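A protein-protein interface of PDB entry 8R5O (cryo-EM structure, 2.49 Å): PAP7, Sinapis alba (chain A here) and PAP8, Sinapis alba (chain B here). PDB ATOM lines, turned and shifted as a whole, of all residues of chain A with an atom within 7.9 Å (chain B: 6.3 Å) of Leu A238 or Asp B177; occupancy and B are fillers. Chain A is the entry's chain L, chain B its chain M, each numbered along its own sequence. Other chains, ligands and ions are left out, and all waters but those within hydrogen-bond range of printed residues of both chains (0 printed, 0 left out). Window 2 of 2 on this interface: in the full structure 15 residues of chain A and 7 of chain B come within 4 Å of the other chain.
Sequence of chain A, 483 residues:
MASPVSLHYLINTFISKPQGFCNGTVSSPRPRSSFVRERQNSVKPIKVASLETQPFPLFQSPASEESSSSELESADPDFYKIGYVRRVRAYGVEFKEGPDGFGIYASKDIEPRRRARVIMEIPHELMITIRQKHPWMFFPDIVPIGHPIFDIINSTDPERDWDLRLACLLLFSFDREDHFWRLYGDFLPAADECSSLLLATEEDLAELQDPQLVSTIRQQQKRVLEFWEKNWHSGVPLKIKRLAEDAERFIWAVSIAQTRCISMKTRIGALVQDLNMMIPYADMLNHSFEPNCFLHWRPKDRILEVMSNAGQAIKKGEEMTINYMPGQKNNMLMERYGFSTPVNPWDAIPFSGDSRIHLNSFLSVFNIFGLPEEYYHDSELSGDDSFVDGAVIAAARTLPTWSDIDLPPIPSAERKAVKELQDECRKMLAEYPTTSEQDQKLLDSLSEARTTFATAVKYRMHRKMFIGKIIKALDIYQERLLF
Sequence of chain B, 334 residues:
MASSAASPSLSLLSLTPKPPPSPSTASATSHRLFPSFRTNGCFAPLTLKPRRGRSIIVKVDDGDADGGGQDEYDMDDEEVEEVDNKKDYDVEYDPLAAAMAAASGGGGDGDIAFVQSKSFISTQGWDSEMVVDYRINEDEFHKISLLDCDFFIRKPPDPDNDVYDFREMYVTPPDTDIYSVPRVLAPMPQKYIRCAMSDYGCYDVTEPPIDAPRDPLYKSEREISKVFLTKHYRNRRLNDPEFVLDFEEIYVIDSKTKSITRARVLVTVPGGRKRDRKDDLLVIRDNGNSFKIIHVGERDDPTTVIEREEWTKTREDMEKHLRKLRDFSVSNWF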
ATOM      1  N   PRO A 148     -11.252   6.268  24.192  1.00  0.00           N
ATOM      2  CA  PRO A 148     -10.077   5.519  23.720  1.00  0.00           C
ATOM      3  C   PRO A 148      -8.749   6.222  23.958  1.00  0.00           C
ATOM      4  O   PRO A 148      -7.705   5.572  23.832  1.00  0.00           O
ATOM      5  CB  PRO A 148     -10.350   5.344  22.219  1.00  0.00           C
ATOM      6  CG  PRO A 148     -11.315   6.425  21.879  1.00  0.00           C
ATOM      7  CD  PRO A 148     -12.167   6.609  23.092  1.00  0.00           C
ATOM      8  N   ASP A 175      -9.110  19.415  21.245  1.00  0.00           N
ATOM      9  CA  ASP A 175     -10.336  18.976  20.599  1.00  0.00           C
ATOM     10  C   ASP A 175     -11.582  19.296  21.413  1.00  0.00           C
ATOM     11  O   ASP A 175     -12.687  19.255  20.864  1.00  0.00           O
ATOM     12  CB  ASP A 175     -10.266  17.471  20.328  1.00  0.00           C
ATOM     13  CG  ASP A 175     -11.318  17.005  19.343  1.00  0.00           C
ATOM     14  OD1 ASP A 175     -11.230  17.377  18.155  1.00  0.00           O
ATOM     15  OD2 ASP A 175     -12.229  16.259  19.756  1.00  0.00           O
ATOM     16  N   TRP A 232      -2.098   5.511  16.021  1.00  0.00           N
ATOM     17  CA  TRP A 232      -2.895   6.294  15.088  1.00  0.00           C
ATOM     18  C   TRP A 232      -2.909   5.639  13.715  1.00  0.00           C
ATOM     19  O   TRP A 232      -2.716   6.310  12.696  1.00  0.00           O
ATOM     20  CB  TRP A 232      -2.370   7.727  14.990  1.00  0.00           C
ATOM     21  CG  TRP A 232      -2.997   8.663  15.968  1.00  0.00           C
ATOM     22  CD1 TRP A 232      -4.072   9.471  15.752  1.00  0.00           C
ATOM     23  CD2 TRP A 232      -2.590   8.890  17.322  1.00  0.00           C
ATOM     24  NE1 TRP A 232      -4.361  10.188  16.885  1.00  0.00           N
ATOM     25  CE2 TRP A 232      -3.465   9.851  17.864  1.00  0.00           C
ATOM     26  CE3 TRP A 232      -1.569   8.378  18.127  1.00  0.00           C
ATOM     27  CZ2 TRP A 232      -3.351  10.308  19.174  1.00  0.00           C
ATOM     28  CZ3 TRP A 232      -1.459   8.832  19.424  1.00  0.00           C
ATOM     29  CH2 TRP A 232      -2.344   9.787  19.936  1.00  0.00           C
ATOM     30  N   SER A 234      -4.896   3.037  10.756  1.00  0.00           N
ATOM     31  CA  SER A 234      -6.104   3.276   9.975  1.00  0.00           C
ATOM     32  C   SER A 234      -7.374   2.855  10.707  1.00  0.00           C
ATOM     33  O   SER A 234      -8.438   3.436  10.466  1.00  0.00           O
ATOM     34  CB  SER A 234      -6.010   2.546   8.635  1.00  0.00           C
ATOM     35  OG  SER A 234      -4.865   2.964   7.914  1.00  0.00           O
ATOM     36  N   GLY A 235      -7.294   1.865  11.588  1.00  0.00           N
ATOM     37  CA  GLY A 235      -8.486   1.342  12.222  1.00  0.00           C
ATOM     38  C   GLY A 235      -8.970   2.060  13.460  1.00  0.00           C
ATOM     39  O   GLY A 235      -9.984   1.651  14.032  1.00  0.00           O
ATOM     40  N   VAL A 236      -8.293   3.117  13.897  1.00  0.00           N
ATOM     41  CA  VAL A 236      -8.655   3.800  15.138  1.00  0.00           C
ATOM     42  C   VAL A 236      -9.913   4.632  14.914  1.00  0.00           C
ATOM     43  O   VAL A 236     -10.218   4.996  13.769  1.00  0.00           O
ATOM     44  CB  VAL A 236      -7.490   4.662  15.656  1.00  0.00           C
ATOM     45  CG1 VAL A 236      -6.234   3.824  15.778  1.00  0.00           C
ATOM     46  CG2 VAL A 236      -7.253   5.845  14.748  1.00  0.00           C
ATOM     47  N   PRO A 237     -10.674   4.944  15.962  1.00  0.00           N
ATOM     48  CA  PRO A 237     -11.893   5.738  15.783  1.00  0.00           C
ATOM     49  C   PRO A 237     -11.593   7.153  15.314  1.00  0.00           C
ATOM     50  O   PRO A 237     -10.480   7.666  15.447  1.00  0.00           O
ATOM     51  CB  PRO A 237     -12.523   5.746  17.182  1.00  0.00           C
ATOM     52  CG  PRO A 237     -11.933   4.565  17.873  1.00  0.00           C
ATOM     53  CD  PRO A 237     -10.542   4.449  17.343  1.00  0.00           C
ATOM     54  N   LEU A 238     -12.625   7.784  14.747  1.00  0.00           N
ATOM     55  CA  LEU A 238     -12.483   9.146  14.245  1.00  0.00           C
ATOM     56  C   LEU A 238     -12.133  10.127  15.356  1.00  0.00           C
ATOM     57  O   LEU A 238     -11.374  11.075  15.127  1.00  0.00           O
ATOM     58  CB  LEU A 238     -13.764   9.582  13.538  1.00  0.00           C
ATOM     59  CG  LEU A 238     -13.789  11.026  13.032  1.00  0.00           C
ATOM     60  CD1 LEU A 238     -12.648  11.273  12.056  1.00  0.00           C
ATOM     61  CD2 LEU A 238     -15.123  11.341  12.391  1.00  0.00           C
ATOM     62  N   LYS A 239     -12.670   9.924  16.561  1.00  0.00           N
ATOM     63  CA  LYS A 239     -12.333  10.807  17.672  1.00  0.00           C
ATOM     64  C   LYS A 239     -10.863  10.709  18.058  1.00  0.00           C
ATOM     65  O   LYS A 239     -10.366  11.583  18.775  1.00  0.00           O
ATOM     66  CB  LYS A 239     -13.213  10.500  18.886  1.00  0.00           C
ATOM     67  CG  LYS A 239     -12.961   9.146  19.521  1.00  0.00           C
ATOM     68  CD  LYS A 239     -13.715   9.007  20.832  1.00  0.00           C
ATOM     69  CE  LYS A 239     -15.212   9.140  20.633  1.00  0.00           C
ATOM     70  NZ  LYS A 239     -15.753   8.050  19.782  1.00  0.00           N
ATOM     71  N   ILE A 240     -10.167   9.671  17.606  1.00  0.00           N
ATOM     72  CA  ILE A 240      -8.724   9.563  17.791  1.00  0.00           C
ATOM     73  C   ILE A 240      -7.973  10.118  16.589  1.00  0.00           C
ATOM     74  O   ILE A 240      -6.959  10.804  16.743  1.00  0.00           O
ATOM     75  CB  ILE A 240      -8.335   8.096  18.075  1.00  0.00           C
ATOM     76  CG1 ILE A 240      -8.934   7.634  19.402  1.00  0.00           C
ATOM     77  CG2 ILE A 240      -6.826   7.931  18.096  1.00  0.00           C
ATOM     78  CD1 ILE A 240      -8.502   8.461  20.590  1.00  0.00           C
ATOM     79  N   LYS A 241      -8.460   9.835  15.377  1.00  0.00           N
ATOM     80  CA  LYS A 241      -7.793  10.315  14.171  1.00  0.00           C
ATOM     81  C   LYS A 241      -7.687  11.832  14.153  1.00  0.00           C
ATOM     82  O   LYS A 241      -6.640  12.384  13.801  1.00  0.00           O
ATOM     83  CB  LYS A 241      -8.538   9.845  12.921  1.00  0.00           C
ATOM     84  CG  LYS A 241      -8.563   8.354  12.707  1.00  0.00           C
ATOM     85  CD  LYS A 241      -8.549   8.033  11.223  1.00  0.00           C
ATOM     86  CE  LYS A 241      -8.876   6.576  10.960  1.00  0.00           C
ATOM     87  NZ  LYS A 241     -10.309   6.271  11.223  1.00  0.00           N
ATOM     88  N   ARG A 242      -8.765  12.524  14.523  1.00  0.00           N
ATOM     89  CA  ARG A 242      -8.791  13.976  14.421  1.00  0.00           C
ATOM     90  C   ARG A 242      -7.861  14.660  15.415  1.00  0.00           C
ATOM     91  O   ARG A 242      -7.640  15.868  15.290  1.00  0.00           O
ATOM     92  CB  ARG A 242     -10.220  14.493  14.596  1.00  0.00           C
ATOM     93  CG  ARG A 242     -10.857  14.197  15.941  1.00  0.00           C
ATOM     94  CD  ARG A 242     -12.168  14.953  16.076  1.00  0.00           C
ATOM     95  NE  ARG A 242     -12.773  14.807  17.393  1.00  0.00           N
ATOM     96  CZ  ARG A 242     -13.827  14.047  17.656  1.00  0.00           C
ATOM     97  NH1 ARG A 242     -14.425  13.345  16.709  1.00  0.00           N
ATOM     98  NH2 ARG A 242     -14.294  13.994  18.899  1.00  0.00           N
ATOM     99  N   LEU A 243      -7.314  13.927  16.386  1.00  0.00           N
ATOM    100  CA  LEU A 243      -6.352  14.520  17.309  1.00  0.00           C
ATOM    101  C   LEU A 243      -5.005  14.740  16.630  1.00  0.00           C
ATOM    102  O   LEU A 243      -4.463  15.851  16.645  1.00  0.00           O
ATOM    103  CB  LEU A 243      -6.189  13.633  18.542  1.00  0.00           C
ATOM    104  CG  LEU A 243      -7.450  13.341  19.352  1.00  0.00           C
ATOM    105  CD1 LEU A 243      -7.094  12.648  20.654  1.00  0.00           C
ATOM    106  CD2 LEU A 243      -8.216  14.619  19.615  1.00  0.00           C
ATOM    107  N   ALA A 244      -4.450  13.690  16.029  1.00  0.00           N
ATOM    108  CA  ALA A 244      -3.156  13.746  15.350  1.00  0.00           C
ATOM    109  C   ALA A 244      -3.342  13.134  13.967  1.00  0.00           C
ATOM    110  O   ALA A 244      -3.106  11.939  13.769  1.00  0.00           O
ATOM    111  CB  ALA A 244      -2.078  13.025  16.151  1.00  0.00           C
ATOM    112  N   TYR B 134     -18.995   0.026   6.473  1.00  0.00           N
ATOM    113  CA  TYR B 134     -17.911   0.955   6.191  1.00  0.00           C
ATOM    114  C   TYR B 134     -18.039   2.202   7.061  1.00  0.00           C
ATOM    115  O   TYR B 134     -19.015   2.387   7.793  1.00  0.00           O
ATOM    116  CB  TYR B 134     -17.901   1.328   4.706  1.00  0.00           C
ATOM    117  CG  TYR B 134     -19.240   1.817   4.202  1.00  0.00           C
ATOM    118  CD1 TYR B 134     -20.175   0.930   3.687  1.00  0.00           C
ATOM    119  CD2 TYR B 134     -19.570   3.165   4.248  1.00  0.00           C
ATOM    120  CE1 TYR B 134     -21.400   1.372   3.231  1.00  0.00           C
ATOM    121  CE2 TYR B 134     -20.791   3.614   3.792  1.00  0.00           C
ATOM    122  CZ  TYR B 134     -21.702   2.713   3.284  1.00  0.00           C
ATOM    123  OH  TYR B 134     -22.921   3.159   2.829  1.00  0.00           O
ATOM    124  N   ARG B 135     -17.029   3.064   6.973  1.00  0.00           N
ATOM    125  CA  ARG B 135     -17.023   4.357   7.642  1.00  0.00           C
ATOM    126  C   ARG B 135     -16.916   5.441   6.583  1.00  0.00           C
ATOM    127  O   ARG B 135     -15.967   5.449   5.790  1.00  0.00           O
ATOM    128  CB  ARG B 135     -15.873   4.461   8.646  1.00  0.00           C
ATOM    129  CG  ARG B 135     -16.021   3.544   9.844  1.00  0.00           C
ATOM    130  CD  ARG B 135     -14.922   3.792  10.858  1.00  0.00           C
ATOM    131  NE  ARG B 135     -13.604   3.498  10.309  1.00  0.00           N
ATOM    132  CZ  ARG B 135     -12.462   3.759  10.929  1.00  0.00           C
ATOM    133  NH1 ARG B 135     -12.438   4.330  12.122  1.00  0.00           N
ATOM    134  NH2 ARG B 135     -11.315   3.442  10.335  1.00  0.00           N
ATOM    135  N   ILE B 136     -17.887   6.354   6.572  1.00  0.00           N
ATOM    136  CA  ILE B 136     -17.952   7.359   5.523  1.00  0.00           C
ATOM    137  C   ILE B 136     -16.880   8.422   5.735  1.00  0.00           C
ATOM    138  O   ILE B 136     -16.330   8.595   6.828  1.00  0.00           O
ATOM    139  CB  ILE B 136     -19.352   7.991   5.467  1.00  0.00           C
ATOM    140  CG1 ILE B 136     -19.598   8.843   6.713  1.00  0.00           C
ATOM    141  CG2 ILE B 136     -20.414   6.918   5.350  1.00  0.00           C
ATOM    142  CD1 ILE B 136     -20.893   9.609   6.673  1.00  0.00           C
ATOM    143  N   GLU B 138     -16.430  11.986   6.323  1.00  0.00           N
ATOM    144  CA  GLU B 138     -17.379  12.950   6.867  1.00  0.00           C
ATOM    145  C   GLU B 138     -17.270  14.338   6.249  1.00  0.00           C
ATOM    146  O   GLU B 138     -18.170  15.157   6.467  1.00  0.00           O
ATOM    147  CB  GLU B 138     -17.218  13.053   8.384  1.00  0.00           C
ATOM    148  CG  GLU B 138     -17.784  11.869   9.148  1.00  0.00           C
ATOM    149  CD  GLU B 138     -17.914  12.144  10.633  1.00  0.00           C
ATOM    150  OE1 GLU B 138     -17.611  13.278  11.056  1.00  0.00           O
ATOM    151  OE2 GLU B 138     -18.319  11.228  11.379  1.00  0.00           O
ATOM    152  N   THR B 172     -25.912   8.457  13.329  1.00  0.00           N
ATOM    153  CA  THR B 172     -24.937   7.892  14.245  1.00  0.00           C
ATOM    154  C   THR B 172     -25.263   8.325  15.666  1.00  0.00           C
ATOM    155  O   THR B 172     -25.840   9.396  15.869  1.00  0.00           O
ATOM    156  CB  THR B 172     -23.519   8.361  13.879  1.00  0.00           C
ATOM    157  OG1 THR B 172     -23.333   8.261  12.464  1.00  0.00           O
ATOM    158  CG2 THR B 172     -22.463   7.524  14.566  1.00  0.00           C
ATOM    159  N   PRO B 173     -24.919   7.515  16.665  1.00  0.00           N
ATOM    160  CA  PRO B 173     -24.901   8.023  18.030  1.00  0.00           C
ATOM    161  C   PRO B 173     -23.894   9.148  18.157  1.00  0.00           C
ATOM    162  O   PRO B 173     -22.890   9.192  17.420  1.00  0.00           O
ATOM    163  CB  PRO B 173     -24.494   6.797  18.861  1.00  0.00           C
ATOM    164  CG  PRO B 173     -24.021   5.771  17.874  1.00  0.00           C
ATOM    165  CD  PRO B 173     -24.774   6.051  16.626  1.00  0.00           C
ATOM    166  N   ASP B 175     -20.983  11.738  18.592  1.00  0.00           N
ATOM    167  CA  ASP B 175     -19.526  11.594  18.596  1.00  0.00           C
ATOM    168  C   ASP B 175     -19.107  10.133  18.447  1.00  0.00           C
ATOM    169  O   ASP B 175     -18.412   9.558  19.284  1.00  0.00           O
ATOM    170  CB  ASP B 175     -18.915  12.215  19.850  1.00  0.00           C
ATOM    171  CG  ASP B 175     -17.475  12.640  19.642  1.00  0.00           C
ATOM    172  OD1 ASP B 175     -17.001  12.582  18.488  1.00  0.00           O
ATOM    173  OD2 ASP B 175     -16.816  13.032  20.626  1.00  0.00           O
ATOM    174  N   THR B 176     -19.549   9.537  17.343  1.00  0.00           N
ATOM    175  CA  THR B 176     -19.242   8.149  17.032  1.00  0.00           C
ATOM    176  C   THR B 176     -19.119   8.023  15.520  1.00  0.00           C
ATOM    177  O   THR B 176     -19.627   8.857  14.768  1.00  0.00           O
ATOM    178  CB  THR B 176     -20.317   7.200  17.586  1.00  0.00           C
ATOM    179  OG1 THR B 176     -20.649   7.585  18.926  1.00  0.00           O
ATOM    180  CG2 THR B 176     -19.828   5.761  17.603  1.00  0.00           C
ATOM    181  N   ASP B 177     -18.419   6.980  15.078  1.00  0.00           N
ATOM    182  CA  ASP B 177     -18.264   6.740  13.649  1.00  0.00           C
ATOM    183  C   ASP B 177     -18.811   5.375  13.252  1.00  0.00           C
ATOM    184  O   ASP B 177     -18.178   4.647  12.480  1.00  0.00           O
ATOM    185  CB  ASP B 177     -16.795   6.877  13.237  1.00  0.00           C
ATOM    186  CG  ASP B 177     -15.859   6.087  14.129  1.00  0.00           C
ATOM    187  OD1 ASP B 177     -16.328   5.511  15.133  1.00  0.00           O
ATOM    188  OD2 ASP B 177     -14.650   6.040  13.824  1.00  0.00           O
ATOM    189  N   ILE B 178     -19.985   5.022  13.767  1.00  0.00           N
ATOM    190  CA  ILE B 178     -20.685   3.795  13.400  1.00  0.00           C
ATOM    191  C   ILE B 178     -22.013   4.208  12.781  1.00  0.00           C
ATOM    192  O   ILE B 178     -22.944   4.597  13.497  1.00  0.00           O
ATOM    193  CB  ILE B 178     -20.897   2.868  14.603  1.00  0.00           C
ATOM    194  CG1 ILE B 178     -19.562   2.590  15.293  1.00  0.00           C
ATOM    195  CG2 ILE B 178     -21.549   1.571  14.161  1.00  0.00           C
ATOM    196  CD1 ILE B 178     -19.682   1.743  16.529  1.00  0.00           C
ATOM    197  N   TYR B 179     -22.111   4.102  11.462  1.00  0.00           N
ATOM    198  CA  TYR B 179     -23.182   4.728  10.703  1.00  0.00           C
ATOM    199  C   TYR B 179     -24.270   3.725  10.343  1.00  0.00           C
ATOM    200  O   TYR B 179     -24.003   2.546  10.101  1.00  0.00           O
ATOM    201  CB  TYR B 179     -22.620   5.376   9.437  1.00  0.00           C
ATOM    202  CG  TYR B 179     -21.506   6.358   9.725  1.00  0.00           C
ATOM    203  CD1 TYR B 179     -20.195   5.930   9.857  1.00  0.00           C
ATOM    204  CD2 TYR B 179     -21.770   7.709   9.883  1.00  0.00           C
ATOM    205  CE1 TYR B 179     -19.178   6.816  10.131  1.00  0.00           C
ATOM    206  CE2 TYR B 179     -20.755   8.604  10.159  1.00  0.00           C
ATOM    207  CZ  TYR B 179     -19.461   8.150  10.281  1.00  0.00           C
ATOM    208  OH  TYR B 179     -18.442   9.028  10.552  1.00  0.00           O
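O of Val A236 sits at hydrogen-bond distance from NH1 of Arg B135, at 2.8 Å.
NH2 of Arg A242 lies within salt-bridge range of OD1 of Asp B175 (3.1 Å).
The side-chain amino group of Lys A241 lies close to the guanidinium group of Arg B135 (3.0 Å).
The guanidinium group (NH2) of Arg B135 is in hydrogen-bond range of the backbone carbonyl oxygen (O) of Ser A234, at 2.9 Å.
The backbone NH of Leu A238 lies within hydrogen-bond range of the side-chain carboxylate of Asp B177, 2.8 Å away.
NZ of Lys A239 lies within hydrogen-bond range of O of Asp B175 (3.1 Å).
Leu A238 touches just these residues of chain B: Glu B138 (3.4 Å) and Asp B177 (2.8 Å).
Of the printed residues of chain A, Asp B177 touches Pro A237 and Leu A238.
Printed residues of chain B within 4 Å of Ser A234: Arg B135.
Printed residues of chain B within 4 Å of Gly A235: Arg B135 (3.997 Å).
Of the printed residues of chain B, Arg A242 touches Asp B175 (3.1 Å).
Asp A175 touches none of the printed residues of chain B.
Tyr B179 touches none of the printed residues of chain A.
The nearest residue of chain B that does not touch Leu A238 is Arg B135 (4.3 Å).
The nearest residue of chain A that does not touch Asp B177 is Val A236 (4.6 Å).
The nearest printed residue of chain B that does not touch Arg A242 is Thr B176 (6.4 Å).
Of the 14 printed residues of chain A, 8 touch a printed residue of chain B.
Of the 11 printed residues of chain B, 4 touch a printed residue of chain A.
Printed residues of chain B that touch a printed residue of chain A: Arg B135, Glu B138, Asp B175 and Asp B177.
Among the printed residues, 10 pairs touch across the chains.
Among the printed residues, Asp or Glu carboxylates within 4 Å of a Lys or Arg side-chain nitrogen of the other chain: Arg A242 with Asp B175.
Among the printed residues, pairs that only touch across the chains: Gly A235 with Arg B135, Pro A237 with Arg B135, Pro A237 with Asp B177 and Leu A238 with Glu B138.
The side-chain amino group (NZ) of Lys A241 lies within hydrogen-bond range of the backbone carbonyl oxygen (O) of Val A236, 2.8 Å away.
NE of Arg A242 is in salt-bridge range of OD2 of Asp A175 (2.8 Å).
NH1 of Arg B135 lies within salt-bridge range of OD2 of Asp B177 (3.3 Å).
The side-chain amino group of Lys A241 sits close to the backbone carbonyl oxygen of Ser A234, at 3.5 Å.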
